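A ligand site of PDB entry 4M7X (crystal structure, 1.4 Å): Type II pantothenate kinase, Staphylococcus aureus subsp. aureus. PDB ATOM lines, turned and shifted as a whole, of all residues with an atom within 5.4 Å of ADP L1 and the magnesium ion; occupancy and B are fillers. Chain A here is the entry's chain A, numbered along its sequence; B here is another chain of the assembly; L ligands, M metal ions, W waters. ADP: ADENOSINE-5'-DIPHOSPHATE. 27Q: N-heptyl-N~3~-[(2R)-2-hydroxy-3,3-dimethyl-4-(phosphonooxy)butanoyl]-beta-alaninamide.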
ATOM      1  N   ASP A   6     -11.131  15.088  -8.021  1.00  0.00           N
ATOM      2  CA  ASP A   6     -12.182  15.386  -8.979  1.00  0.00           C
ATOM      3  C   ASP A   6     -13.407  15.618  -8.084  1.00  0.00           C
ATOM      4  O   ASP A   6     -14.015  14.689  -7.570  1.00  0.00           O
ATOM      5  CB  ASP A   6     -12.378  14.210  -9.941  1.00  0.00           C
ATOM      6  CG  ASP A   6     -13.505  14.411 -10.885  1.00  0.00           C
ATOM      7  OD1 ASP A   6     -14.199  15.423 -10.786  1.00  0.00           O
ATOM      8  OD2 ASP A   6     -13.686  13.566 -11.760  1.00  0.00           O
ATOM      9  N   GLY A   8     -16.819  16.480  -7.994  1.00  0.00           N
ATOM     10  CA  GLY A   8     -17.973  16.506  -8.899  1.00  0.00           C
ATOM     11  C   GLY A   8     -19.253  16.982  -8.250  1.00  0.00           C
ATOM     12  O   GLY A   8     -19.271  17.452  -7.119  1.00  0.00           O
ATOM     13  N   GLY A   9     -20.354  16.817  -8.966  1.00  0.00           N
ATOM     14  CA  GLY A   9     -21.636  17.257  -8.468  1.00  0.00           C
ATOM     15  C   GLY A   9     -22.185  16.485  -7.294  1.00  0.00           C
ATOM     16  O   GLY A   9     -22.924  17.033  -6.502  1.00  0.00           O
ATOM     17  N   THR A  10     -21.825  15.208  -7.182  1.00  0.00           N
ATOM     18  CA  THR A  10     -22.307  14.354  -6.079  1.00  0.00           C
ATOM     19  C   THR A  10     -21.182  13.735  -5.268  1.00  0.00           C
ATOM     20  O   THR A  10     -21.299  13.671  -4.031  1.00  0.00           O
ATOM     21  CB  THR A  10     -23.231  13.255  -6.608  1.00  0.00           C
ATOM     22  OG1 THR A  10     -24.273  13.869  -7.362  1.00  0.00           O
ATOM     23  CG2 THR A  10     -23.847  12.429  -5.472  1.00  0.00           C
ATOM     24  N   LEU A  11     -20.116  13.281  -5.927  1.00  0.00           N
ATOM     25  CA  LEU A  11     -19.005  12.674  -5.222  1.00  0.00           C
ATOM     26  C   LEU A  11     -17.715  13.394  -5.507  1.00  0.00           C
ATOM     27  O   LEU A  11     -17.478  13.897  -6.625  1.00  0.00           O
ATOM     28  CB  LEU A  11     -18.807  11.225  -5.598  1.00  0.00           C
ATOM     29  CG  LEU A  11     -20.030  10.313  -5.393  1.00  0.00           C
ATOM     30  CD1 LEU A  11     -19.744   8.914  -5.851  1.00  0.00           C
ATOM     31  CD2 LEU A  11     -20.501  10.334  -3.966  1.00  0.00           C
ATOM     32  N   ILE A  12     -16.878  13.448  -4.483  1.00  0.00           N
ATOM     33  CA  ILE A  12     -15.522  13.878  -4.590  1.00  0.00           C
ATOM     34  C   ILE A  12     -14.637  12.639  -4.626  1.00  0.00           C
ATOM     35  O   ILE A  12     -14.638  11.851  -3.699  1.00  0.00           O
ATOM     36  CB  ILE A  12     -15.143  14.772  -3.406  1.00  0.00           C
ATOM     37  CG1 ILE A  12     -16.051  16.018  -3.337  1.00  0.00           C
ATOM     38  CG2 ILE A  12     -13.664  15.171  -3.493  1.00  0.00           C
ATOM     39  CD1 ILE A  12     -15.969  16.793  -2.063  1.00  0.00           C
ATOM     40  N   LYS A  13     -13.855  12.484  -5.696  1.00  0.00           N
ATOM     41  CA  LYS A  13     -12.993  11.348  -5.921  1.00  0.00           C
ATOM     42  C   LYS A  13     -11.587  11.803  -5.676  1.00  0.00           C
ATOM     43  O   LYS A  13     -11.128  12.792  -6.298  1.00  0.00           O
ATOM     44  CB  LYS A  13     -13.097  10.837  -7.382  1.00  0.00           C
ATOM     45  CG  LYS A  13     -14.290   9.950  -7.664  1.00  0.00           C
ATOM     46  CD  LYS A  13     -15.614  10.660  -7.680  1.00  0.00           C
ATOM     47  CE  LYS A  13     -15.661  11.740  -8.760  1.00  0.00           C
ATOM     48  NZ  LYS A  13     -17.014  12.321  -8.917  1.00  0.00           N
ATOM     49  N   LEU A  28     -18.761  12.327  -0.148  1.00  0.00           N
ATOM     50  CA  LEU A  28     -19.881  13.081  -0.749  1.00  0.00           C
ATOM     51  C   LEU A  28     -19.511  14.553  -0.918  1.00  0.00           C
ATOM     52  O   LEU A  28     -18.905  15.183  -0.039  1.00  0.00           O
ATOM     53  CB  LEU A  28     -21.130  12.970   0.161  1.00  0.00           C
ATOM     54  CG  LEU A  28     -21.664  11.572   0.418  1.00  0.00           C
ATOM     55  CD1 LEU A  28     -22.840  11.707   1.375  1.00  0.00           C
ATOM     56  CD2 LEU A  28     -22.101  10.856  -0.838  1.00  0.00           C
ATOM     57  N   THR A  29     -19.909  15.122  -2.038  1.00  0.00           N
ATOM     58  CA  THR A  29     -19.748  16.547  -2.269  1.00  0.00           C
ATOM     59  C   THR A  29     -20.408  17.395  -1.178  1.00  0.00           C
ATOM     60  O   THR A  29     -19.891  18.453  -0.796  1.00  0.00           O
ATOM     61  CB  THR A  29     -20.270  16.912  -3.685  1.00  0.00           C
ATOM     62  OG1 THR A  29     -19.507  16.170  -4.635  1.00  0.00           O
ATOM     63  CG2 THR A  29     -20.146  18.405  -3.922  1.00  0.00           C
ATOM     64  N   GLU A  70     -12.416  19.297 -16.605  1.00  0.00           N
ATOM     65  CA  GLU A  70     -12.728  17.917 -16.317  1.00  0.00           C
ATOM     66  C   GLU A  70     -12.721  17.067 -17.537  1.00  0.00           C
ATOM     67  O   GLU A  70     -12.436  15.894 -17.430  1.00  0.00           O
ATOM     68  CB  GLU A  70     -14.056  17.722 -15.515  1.00  0.00           C
ATOM     69  CG  GLU A  70     -15.354  18.042 -16.239  1.00  0.00           C
ATOM     70  CD  GLU A  70     -16.581  17.674 -15.408  1.00  0.00           C
ATOM     71  OE1 GLU A  70     -17.012  16.494 -15.426  1.00  0.00           O
ATOM     72  OE2 GLU A  70     -17.119  18.564 -14.729  1.00  0.00           O
ATOM     73  N   ASN A  96     -19.438   9.375 -19.711  1.00  0.00           N
ATOM     74  CA  ASN A  96     -19.147   9.663 -18.324  1.00  0.00           C
ATOM     75  C   ASN A  96     -20.497   9.851 -17.650  1.00  0.00           C
ATOM     76  O   ASN A  96     -21.087  10.938 -17.729  1.00  0.00           O
ATOM     77  CB  ASN A  96     -18.239  10.893 -18.243  1.00  0.00           C
ATOM     78  CG  ASN A  96     -17.702  11.133 -16.874  1.00  0.00           C
ATOM     79  OD1 ASN A  96     -18.128  10.498 -15.909  1.00  0.00           O
ATOM     80  ND2 ASN A  96     -16.763  12.093 -16.759  1.00  0.00           N
ATOM     81  N   VAL A  97     -20.933   8.812 -16.968  1.00  0.00           N
ATOM     82  CA  VAL A  97     -22.270   8.792 -16.364  1.00  0.00           C
ATOM     83  C   VAL A  97     -22.107   9.138 -14.902  1.00  0.00           C
ATOM     84  O   VAL A  97     -21.966   8.263 -14.031  1.00  0.00           O
ATOM     85  CB  VAL A  97     -22.910   7.417 -16.554  1.00  0.00           C
ATOM     86  CG1 VAL A  97     -24.328   7.454 -16.086  1.00  0.00           C
ATOM     87  CG2 VAL A  97     -22.826   6.982 -18.014  1.00  0.00           C
ATOM     88  N   GLY A  98     -22.083  10.428 -14.655  1.00  0.00           N
ATOM     89  CA  GLY A  98     -21.924  10.998 -13.333  1.00  0.00           C
ATOM     90  C   GLY A  98     -23.238  11.444 -12.807  1.00  0.00           C
ATOM     91  O   GLY A  98     -24.258  10.771 -13.026  1.00  0.00           O
ATOM     92  N   THR A  99     -23.274  12.619 -12.162  1.00  0.00           N
ATOM     93  CA  THR A  99     -24.524  13.183 -11.740  1.00  0.00           C
ATOM     94  C   THR A  99     -25.440  13.339 -12.970  1.00  0.00           C
ATOM     95  O   THR A  99     -26.613  13.017 -12.911  1.00  0.00           O
ATOM     96  CB  THR A  99     -24.324  14.516 -11.029  1.00  0.00           C
ATOM     97  OG1 THR A  99     -23.439  14.310  -9.874  1.00  0.00           O
ATOM     98  CG2 THR A  99     -25.593  15.028 -10.541  1.00  0.00           C
ATOM     99  N   GLY A 100     -24.855  13.830 -14.046  1.00  0.00           N
ATOM    100  CA  GLY A 100     -25.422  13.767 -15.371  1.00  0.00           C
ATOM    101  C   GLY A 100     -24.451  13.103 -16.331  1.00  0.00           C
ATOM    102  O   GLY A 100     -23.367  12.692 -15.907  1.00  0.00           O
ATOM    103  N   GLY A 121     -26.760   9.500 -12.886  1.00  0.00           N
ATOM    104  CA  GLY A 121     -26.877   9.121 -11.494  1.00  0.00           C
ATOM    105  C   GLY A 121     -27.764   9.996 -10.641  1.00  0.00           C
ATOM    106  O   GLY A 121     -28.380   9.557  -9.703  1.00  0.00           O
ATOM    107  N   GLY A 122     -27.774  11.298 -10.913  1.00  0.00           N
ATOM    108  CA  GLY A 122     -28.613  12.220 -10.169  1.00  0.00           C
ATOM    109  C   GLY A 122     -30.101  11.937 -10.346  1.00  0.00           C
ATOM    110  O   GLY A 122     -30.873  12.057  -9.393  1.00  0.00           O
ATOM    111  N   ILE A 124     -31.271   8.887 -11.123  1.00  0.00           N
ATOM    112  CA  ILE A 124     -31.498   7.643 -10.389  1.00  0.00           C
ATOM    113  C   ILE A 124     -31.811   7.978  -8.924  1.00  0.00           C
ATOM    114  O   ILE A 124     -32.808   7.506  -8.345  1.00  0.00           O
ATOM    115  CB  ILE A 124     -30.301   6.715 -10.538  1.00  0.00           C
ATOM    116  CG1 ILE A 124     -30.219   6.228 -11.955  1.00  0.00           C
ATOM    117  CG2 ILE A 124     -30.398   5.566  -9.561  1.00  0.00           C
ATOM    118  CD1 ILE A 124     -28.992   5.398 -12.281  1.00  0.00           C
ATOM    119  N   GLN A 125     -30.971   8.816  -8.317  1.00  0.00           N
ATOM    120  CA  GLN A 125     -31.225   9.188  -6.905  1.00  0.00           C
ATOM    121  C   GLN A 125     -32.500  10.007  -6.685  1.00  0.00           C
ATOM    122  O   GLN A 125     -33.238   9.779  -5.764  1.00  0.00           O
ATOM    123  CB  GLN A 125     -30.053   9.944  -6.297  1.00  0.00           C
ATOM    124  CG  GLN A 125     -28.799   9.135  -6.203  1.00  0.00           C
ATOM    125  CD  GLN A 125     -27.714   9.852  -5.536  1.00  0.00           C
ATOM    126  OE1 GLN A 125     -26.961  10.637  -6.194  1.00  0.00           O
ATOM    127  NE2 GLN A 125     -27.595   9.636  -4.237  1.00  0.00           N
ATOM    128  N   TYR A 137     -28.094   5.697  -0.848  1.00  0.00           N
ATOM    129  CA  TYR A 137     -27.711   5.234  -2.191  1.00  0.00           C
ATOM    130  C   TYR A 137     -27.617   3.677  -2.248  1.00  0.00           C
ATOM    131  O   TYR A 137     -28.117   3.057  -3.175  1.00  0.00           O
ATOM    132  CB  TYR A 137     -26.372   5.832  -2.623  1.00  0.00           C
ATOM    133  CG  TYR A 137     -25.958   5.321  -3.973  1.00  0.00           C
ATOM    134  CD1 TYR A 137     -26.554   5.803  -5.115  1.00  0.00           C
ATOM    135  CD2 TYR A 137     -24.989   4.323  -4.102  1.00  0.00           C
ATOM    136  CE1 TYR A 137     -26.206   5.334  -6.337  1.00  0.00           C
ATOM    137  CE2 TYR A 137     -24.621   3.855  -5.335  1.00  0.00           C
ATOM    138  CZ  TYR A 137     -25.231   4.366  -6.459  1.00  0.00           C
ATOM    139  OH  TYR A 137     -24.900   3.925  -7.678  1.00  0.00           O
ATOM    140  N   GLY A 224     -17.980   6.301 -14.673  1.00  0.00           N
ATOM    141  CA  GLY A 224     -18.799   7.080 -13.769  1.00  0.00           C
ATOM    142  C   GLY A 224     -19.219   6.309 -12.569  1.00  0.00           C
ATOM    143  O   GLY A 224     -19.404   5.068 -12.570  1.00  0.00           O
ATOM    144  N   SER A 225     -19.436   7.024 -11.491  1.00  0.00           N
ATOM    145  CA  SER A 225     -19.788   6.389 -10.281  1.00  0.00           C
ATOM    146  C   SER A 225     -21.207   5.827 -10.301  1.00  0.00           C
ATOM    147  O   SER A 225     -21.548   5.083  -9.468  1.00  0.00           O
ATOM    148  CB  SER A 225     -19.612   7.305  -9.052  1.00  0.00           C
ATOM    149  OG  SER A 225     -18.298   7.887  -9.005  1.00  0.00           O
ATOM    150  N   SER A 226     -21.998   6.178 -11.307  1.00  0.00           N
ATOM    151  CA  SER A 226     -23.380   5.721 -11.390  1.00  0.00           C
ATOM    152  C   SER A 226     -23.454   4.223 -11.544  1.00  0.00           C
ATOM    153  O   SER A 226     -24.491   3.634 -11.233  1.00  0.00           O
ATOM    154  CB  SER A 226     -24.055   6.348 -12.573  1.00  0.00           C
ATOM    155  OG  SER A 226     -24.180   7.758 -12.368  1.00  0.00           O
ATOM    156  N   HIS A 228     -21.513   2.143  -9.816  1.00  0.00           N
ATOM    157  CA  HIS A 228     -21.117   1.541  -8.566  1.00  0.00           C
ATOM    158  C   HIS A 228     -22.313   0.998  -7.851  1.00  0.00           C
ATOM    159  O   HIS A 228     -23.317   1.710  -7.661  1.00  0.00           O
ATOM    160  CB  HIS A 228     -20.418   2.550  -7.665  1.00  0.00           C
ATOM    161  CG  HIS A 228     -20.078   2.000  -6.303  1.00  0.00           C
ATOM    162  ND1 HIS A 228     -19.221   0.964  -6.123  1.00  0.00           N
ATOM    163  CD2 HIS A 228     -20.538   2.338  -5.047  1.00  0.00           C
ATOM    164  CE1 HIS A 228     -19.128   0.686  -4.834  1.00  0.00           C
ATOM    165  NE2 HIS A 228     -19.923   1.514  -4.165  1.00  0.00           N
ATOM    166  N   ALA A 255     -14.265   5.514 -12.488  1.00  0.00           N
ATOM    167  CA  ALA A 255     -14.820   6.705 -11.867  1.00  0.00           C
ATOM    168  C   ALA A 255     -13.786   7.693 -11.345  1.00  0.00           C
ATOM    169  O   ALA A 255     -14.115   8.811 -11.062  1.00  0.00           O
ATOM    170  CB  ALA A 255     -15.810   6.329 -10.742  1.00  0.00           C
ATOM    171  N   ILE B 159     -23.539  22.983 -10.163  1.00  0.00           N
ATOM    172  CA  ILE B 159     -22.385  22.171  -9.907  1.00  0.00           C
ATOM    173  C   ILE B 159     -21.147  23.030  -9.900  1.00  0.00           C
ATOM    174  O   ILE B 159     -20.328  22.944  -8.997  1.00  0.00           O
ATOM    175  CB  ILE B 159     -22.252  21.026 -10.944  1.00  0.00           C
ATOM    176  CG1 ILE B 159     -23.503  20.144 -10.877  1.00  0.00           C
ATOM    177  CG2 ILE B 159     -20.979  20.225 -10.739  1.00  0.00           C
ATOM    178  CD1 ILE B 159     -23.498  19.028 -11.891  1.00  0.00           C
HETATM  179  PB  ADP L   1     -20.005  13.487 -10.212  1.00  0.00           P
HETATM  180  O1B ADP L   1     -21.087  14.414 -10.762  1.00  0.00           O
HETATM  181  O2B ADP L   1     -18.634  13.641 -10.843  1.00  0.00           O
HETATM  182  O3B ADP L   1     -19.967  13.560  -8.701  1.00  0.00           O
HETATM  183  PA  ADP L   1     -19.926  10.516 -10.375  1.00  0.00           P
HETATM  184  O1A ADP L   1     -19.114  10.501  -9.096  1.00  0.00           O
HETATM  185  O2A ADP L   1     -19.229   9.965 -11.548  1.00  0.00           O
HETATM  186  O3A ADP L   1     -20.453  11.972 -10.562  1.00  0.00           O
HETATM  187  O5' ADP L   1     -21.323   9.800 -10.199  1.00  0.00           O
HETATM  188  C5' ADP L   1     -22.274  10.255  -9.231  1.00  0.00           C
HETATM  189  C4' ADP L   1     -23.363   9.195  -9.117  1.00  0.00           C
HETATM  190  O4' ADP L   1     -22.812   7.955  -8.666  1.00  0.00           O
HETATM  191  C3' ADP L   1     -24.479   9.506  -8.141  1.00  0.00           C
HETATM  192  O3' ADP L   1     -25.423  10.414  -8.695  1.00  0.00           O
HETATM  193  C2' ADP L   1     -25.011   8.117  -7.833  1.00  0.00           C
HETATM  194  O2' ADP L   1     -25.953   7.661  -8.805  1.00  0.00           O
HETATM  195  C1' ADP L   1     -23.751   7.252  -7.886  1.00  0.00           C
HETATM  196  N9  ADP L   1     -23.119   6.949  -6.583  1.00  0.00           N
HETATM  197  C8  ADP L   1     -22.234   5.928  -6.516  1.00  0.00           C
HETATM  198  N7  ADP L   1     -21.842   5.766  -5.232  1.00  0.00           N
HETATM  199  C5  ADP L   1     -22.450   6.678  -4.489  1.00  0.00           C
HETATM  200  C6  ADP L   1     -22.501   7.057  -3.072  1.00  0.00           C
HETATM  201  N6  ADP L   1     -21.729   6.386  -2.167  1.00  0.00           N
HETATM  202  N1  ADP L   1     -23.300   8.053  -2.695  1.00  0.00           N
HETATM  203  C2  ADP L   1     -24.081   8.733  -3.569  1.00  0.00           C
HETATM  204  N3  ADP L   1     -24.103   8.466  -4.892  1.00  0.00           N
HETATM  205  C4  ADP L   1     -23.334   7.450  -5.364  1.00  0.00           C
HETATM  206  OAH 27Q L   2     -20.495  16.248 -12.119  1.00  0.00           O
HETATM  207  PAX 27Q L   2     -20.444  15.638 -13.531  1.00  0.00           P
HETATM  208  OAI 27Q L   2     -21.776  14.786 -14.074  1.00  0.00           O
HETATM  209  OAF 27Q L   2     -19.211  14.759 -13.542  1.00  0.00           O
HETATM  210  OAS 27Q L   2     -20.153  16.807 -14.652  1.00  0.00           O
HETATM  211  CAP 27Q L   2     -20.923  17.930 -14.790  1.00  0.00           C
HETATM  212  CAW 27Q L   2     -21.507  17.989 -16.227  1.00  0.00           C
HETATM  213  CAB 27Q L   2     -20.384  18.223 -17.248  1.00  0.00           C
HETATM  214  CAC 27Q L   2     -22.494  19.150 -16.230  1.00  0.00           C
HETATM  215  CAV 27Q L   2     -22.307  16.665 -16.544  1.00  0.00           C
HETATM  216  OAG 27Q L   2     -23.275  16.363 -15.495  1.00  0.00           O
HETATM  217  CAU 27Q L   2     -23.073  16.775 -17.845  1.00  0.00           C
HETATM  218  OAE 27Q L   2     -22.472  16.816 -18.936  1.00  0.00           O
HETATM  219  NAR 27Q L   2     -24.403  16.820 -17.753  1.00  0.00           N
HETATM  220  CAN 27Q L   2     -25.267  16.878 -18.907  1.00  0.00           C
HETATM  221  CAO 27Q L   2     -25.285  18.357 -19.448  1.00  0.00           C
HETATM  222  CAT 27Q L   2     -25.999  18.392 -20.781  1.00  0.00           C
HETATM  223  OAD 27Q L   2     -25.407  18.170 -21.816  1.00  0.00           O
HETATM  224  NAQ 27Q L   2     -27.302  18.612 -20.764  1.00  0.00           N
HETATM  225  CAM 27Q L   2     -28.073  18.580 -22.008  1.00  0.00           C
HETATM  226  CAL 27Q L   2     -29.546  18.679 -21.766  1.00  0.00           C
HETATM  227  CAK 27Q L   2     -29.801  20.083 -21.408  1.00  0.00           C
HETATM  228  CAJ 27Q L   2     -30.632  20.665 -22.519  1.00  0.00           C
HETATM  229  CAA 27Q L   2     -31.778  21.219 -21.736  1.00  0.00           C
HETATM  230  CAY 27Q L   2     -32.275  22.441 -22.456  1.00  0.00           C
HETATM  231  CAZ 27Q L   2     -32.681  23.410 -21.340  1.00  0.00           C
HETATM  232 MG    MG M   1     -17.732  13.828 -12.687  1.00  0.00          MG
HETATM  233  O   HOH W   1     -16.498  10.021 -11.709  1.00  0.00           O
HETATM  234  O   HOH W   2     -16.782  14.039 -14.532  1.00  0.00           O
HETATM  235  O   HOH W   3     -16.210  12.714 -11.999  1.00  0.00           O
HETATM  236  O   HOH W   4     -24.473   8.861  -0.235  1.00  0.00           O
HETATM  237  O   HOH W   5     -16.696  15.586 -12.049  1.00  0.00           O
HETATM  238  O   HOH W   6     -18.603  12.007 -13.435  1.00  0.00           O
HETATM  239  O   HOH W   7     -26.166  10.847  -1.801  1.00  0.00           O
HETATM  240  O   HOH W   8     -18.918   5.369  -5.081  1.00  0.00           O
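Water W2 lies within hydrogen-bond range of OE1 of Glu 70 (2.6 Å) and ND2 of Asn 96 (3.0 Å).
Water W6 lies within hydrogen-bond range of an oxygen (O2A) of ADP L1 and the side-chain amide oxygen (OD1) of Asn 96.
Water W3 lies within hydrogen-bond range of OD2 of Asp 6 (2.7 Å) and NZ of Lys 13 (3.2 Å).
Water W1 bridges O2A of ADP L1 (2.7 Å) and O of Ala 255 (2.7 Å).
Glu 70 touches the magnesium ion (OE1 to MG, 3.9 Å).
Of the 26 residues printed, 1 comes within 4 Å of the magnesium ion.
OG1 of Thr 29 lies within hydrogen-bond range of N of Leu 11 (3.2 Å).
OG of Ser 226 is in hydrogen-bond range of O of Val 97 (2.8 Å).
The side-chain hydroxyl (OG) of Ser 226 sits close to the backbone NH (N) of Gly 121.
N of Asp 6 sits at hydrogen-bond distance from O of Lys 13 (2.9 Å).
O of Gly 98 is in hydrogen-bond range of OG of Ser 226, 3.1 Å away.
The side-chain hydroxyl (OH) of Tyr 137 is in hydrogen-bond range of the backbone carbonyl oxygen (O) of His 228, 2.7 Å away.
O of Leu 11 is in hydrogen-bond range of NZ of Lys 13.
The side-chain hydroxyl (OG1) of Thr 10 sits at hydrogen-bond distance from the side-chain hydroxyl (OG1) of Thr 99.
Residues that only touch ADP L1: Gly 8, Leu 28, Gly 98, Tyr 137, Gly 224 and His 228.
Hydrophobic or aromatic side chains that line ADP L1: Leu 11, Leu 28, Tyr 137 and His 228.
The backbone NH (N) of Gly 100 is in hydrogen-bond range of an oxygen (OAI) of 27Q L2, at 3.2 Å.
An oxygen (O3') of ADP L1 sits at hydrogen-bond distance from the backbone NH (N) of Gly 122 (3.4 Å).
An oxygen (O3B) of ADP L1 sits at hydrogen-bond distance from the backbone NH of Thr 10 (2.9 Å).
The backbone NH (N) of Ser 226 is in hydrogen-bond range of an oxygen (O4') of ADP L1.
An oxygen (O1B) of ADP L1 is in hydrogen-bond range of the side-chain hydroxyl (OG1) of Thr 99 (2.5 Å).
The backbone NH (N) of Thr 99 is in hydrogen-bond range of an oxygen (O1B) of ADP L1 (3.2 Å).
N of Gly 9 lies within hydrogen-bond range of OAH of 27Q L2 (3.2 Å).
O1B of ADP L1 sits at hydrogen-bond distance from N of Gly 9 (3.1 Å).
NZ of Lys 13 lies within salt-bridge range of O1A of ADP L1, at 2.8 Å.
The backbone NH (N) of Thr 99 is in hydrogen-bond range of an oxygen (OAI) of 27Q L2 (3.3 Å).
The side-chain amide oxygen of Gln 125 is in hydrogen-bond range of an oxygen (O3') of ADP L1 (2.9 Å).
OG of Ser 225 sits at hydrogen-bond distance from O1A of ADP L1.
An oxygen (O2') of ADP L1 sits close to the backbone carbonyl oxygen of Gly 121 (3.2 Å).
N of Leu 11 sits at hydrogen-bond distance from O3B of ADP L1.
An oxygen (O2A) of ADP L1 sits at hydrogen-bond distance from the backbone NH of Ser 225 (2.9 Å).
The magnesium ion is bound by OAF of 27Q L2 (1.9 Å).
Water W3 is bound to the magnesium ion (2.0 Å).
The magnesium ion is bound by O2B of ADP L1.
Water W2 is bound to the magnesium ion, at 2.1 Å.
Water W5 binds the magnesium ion.
Water W6 is bound to the magnesium ion (2.2 Å).
The magnesium ion has six donor atoms within binding distance.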
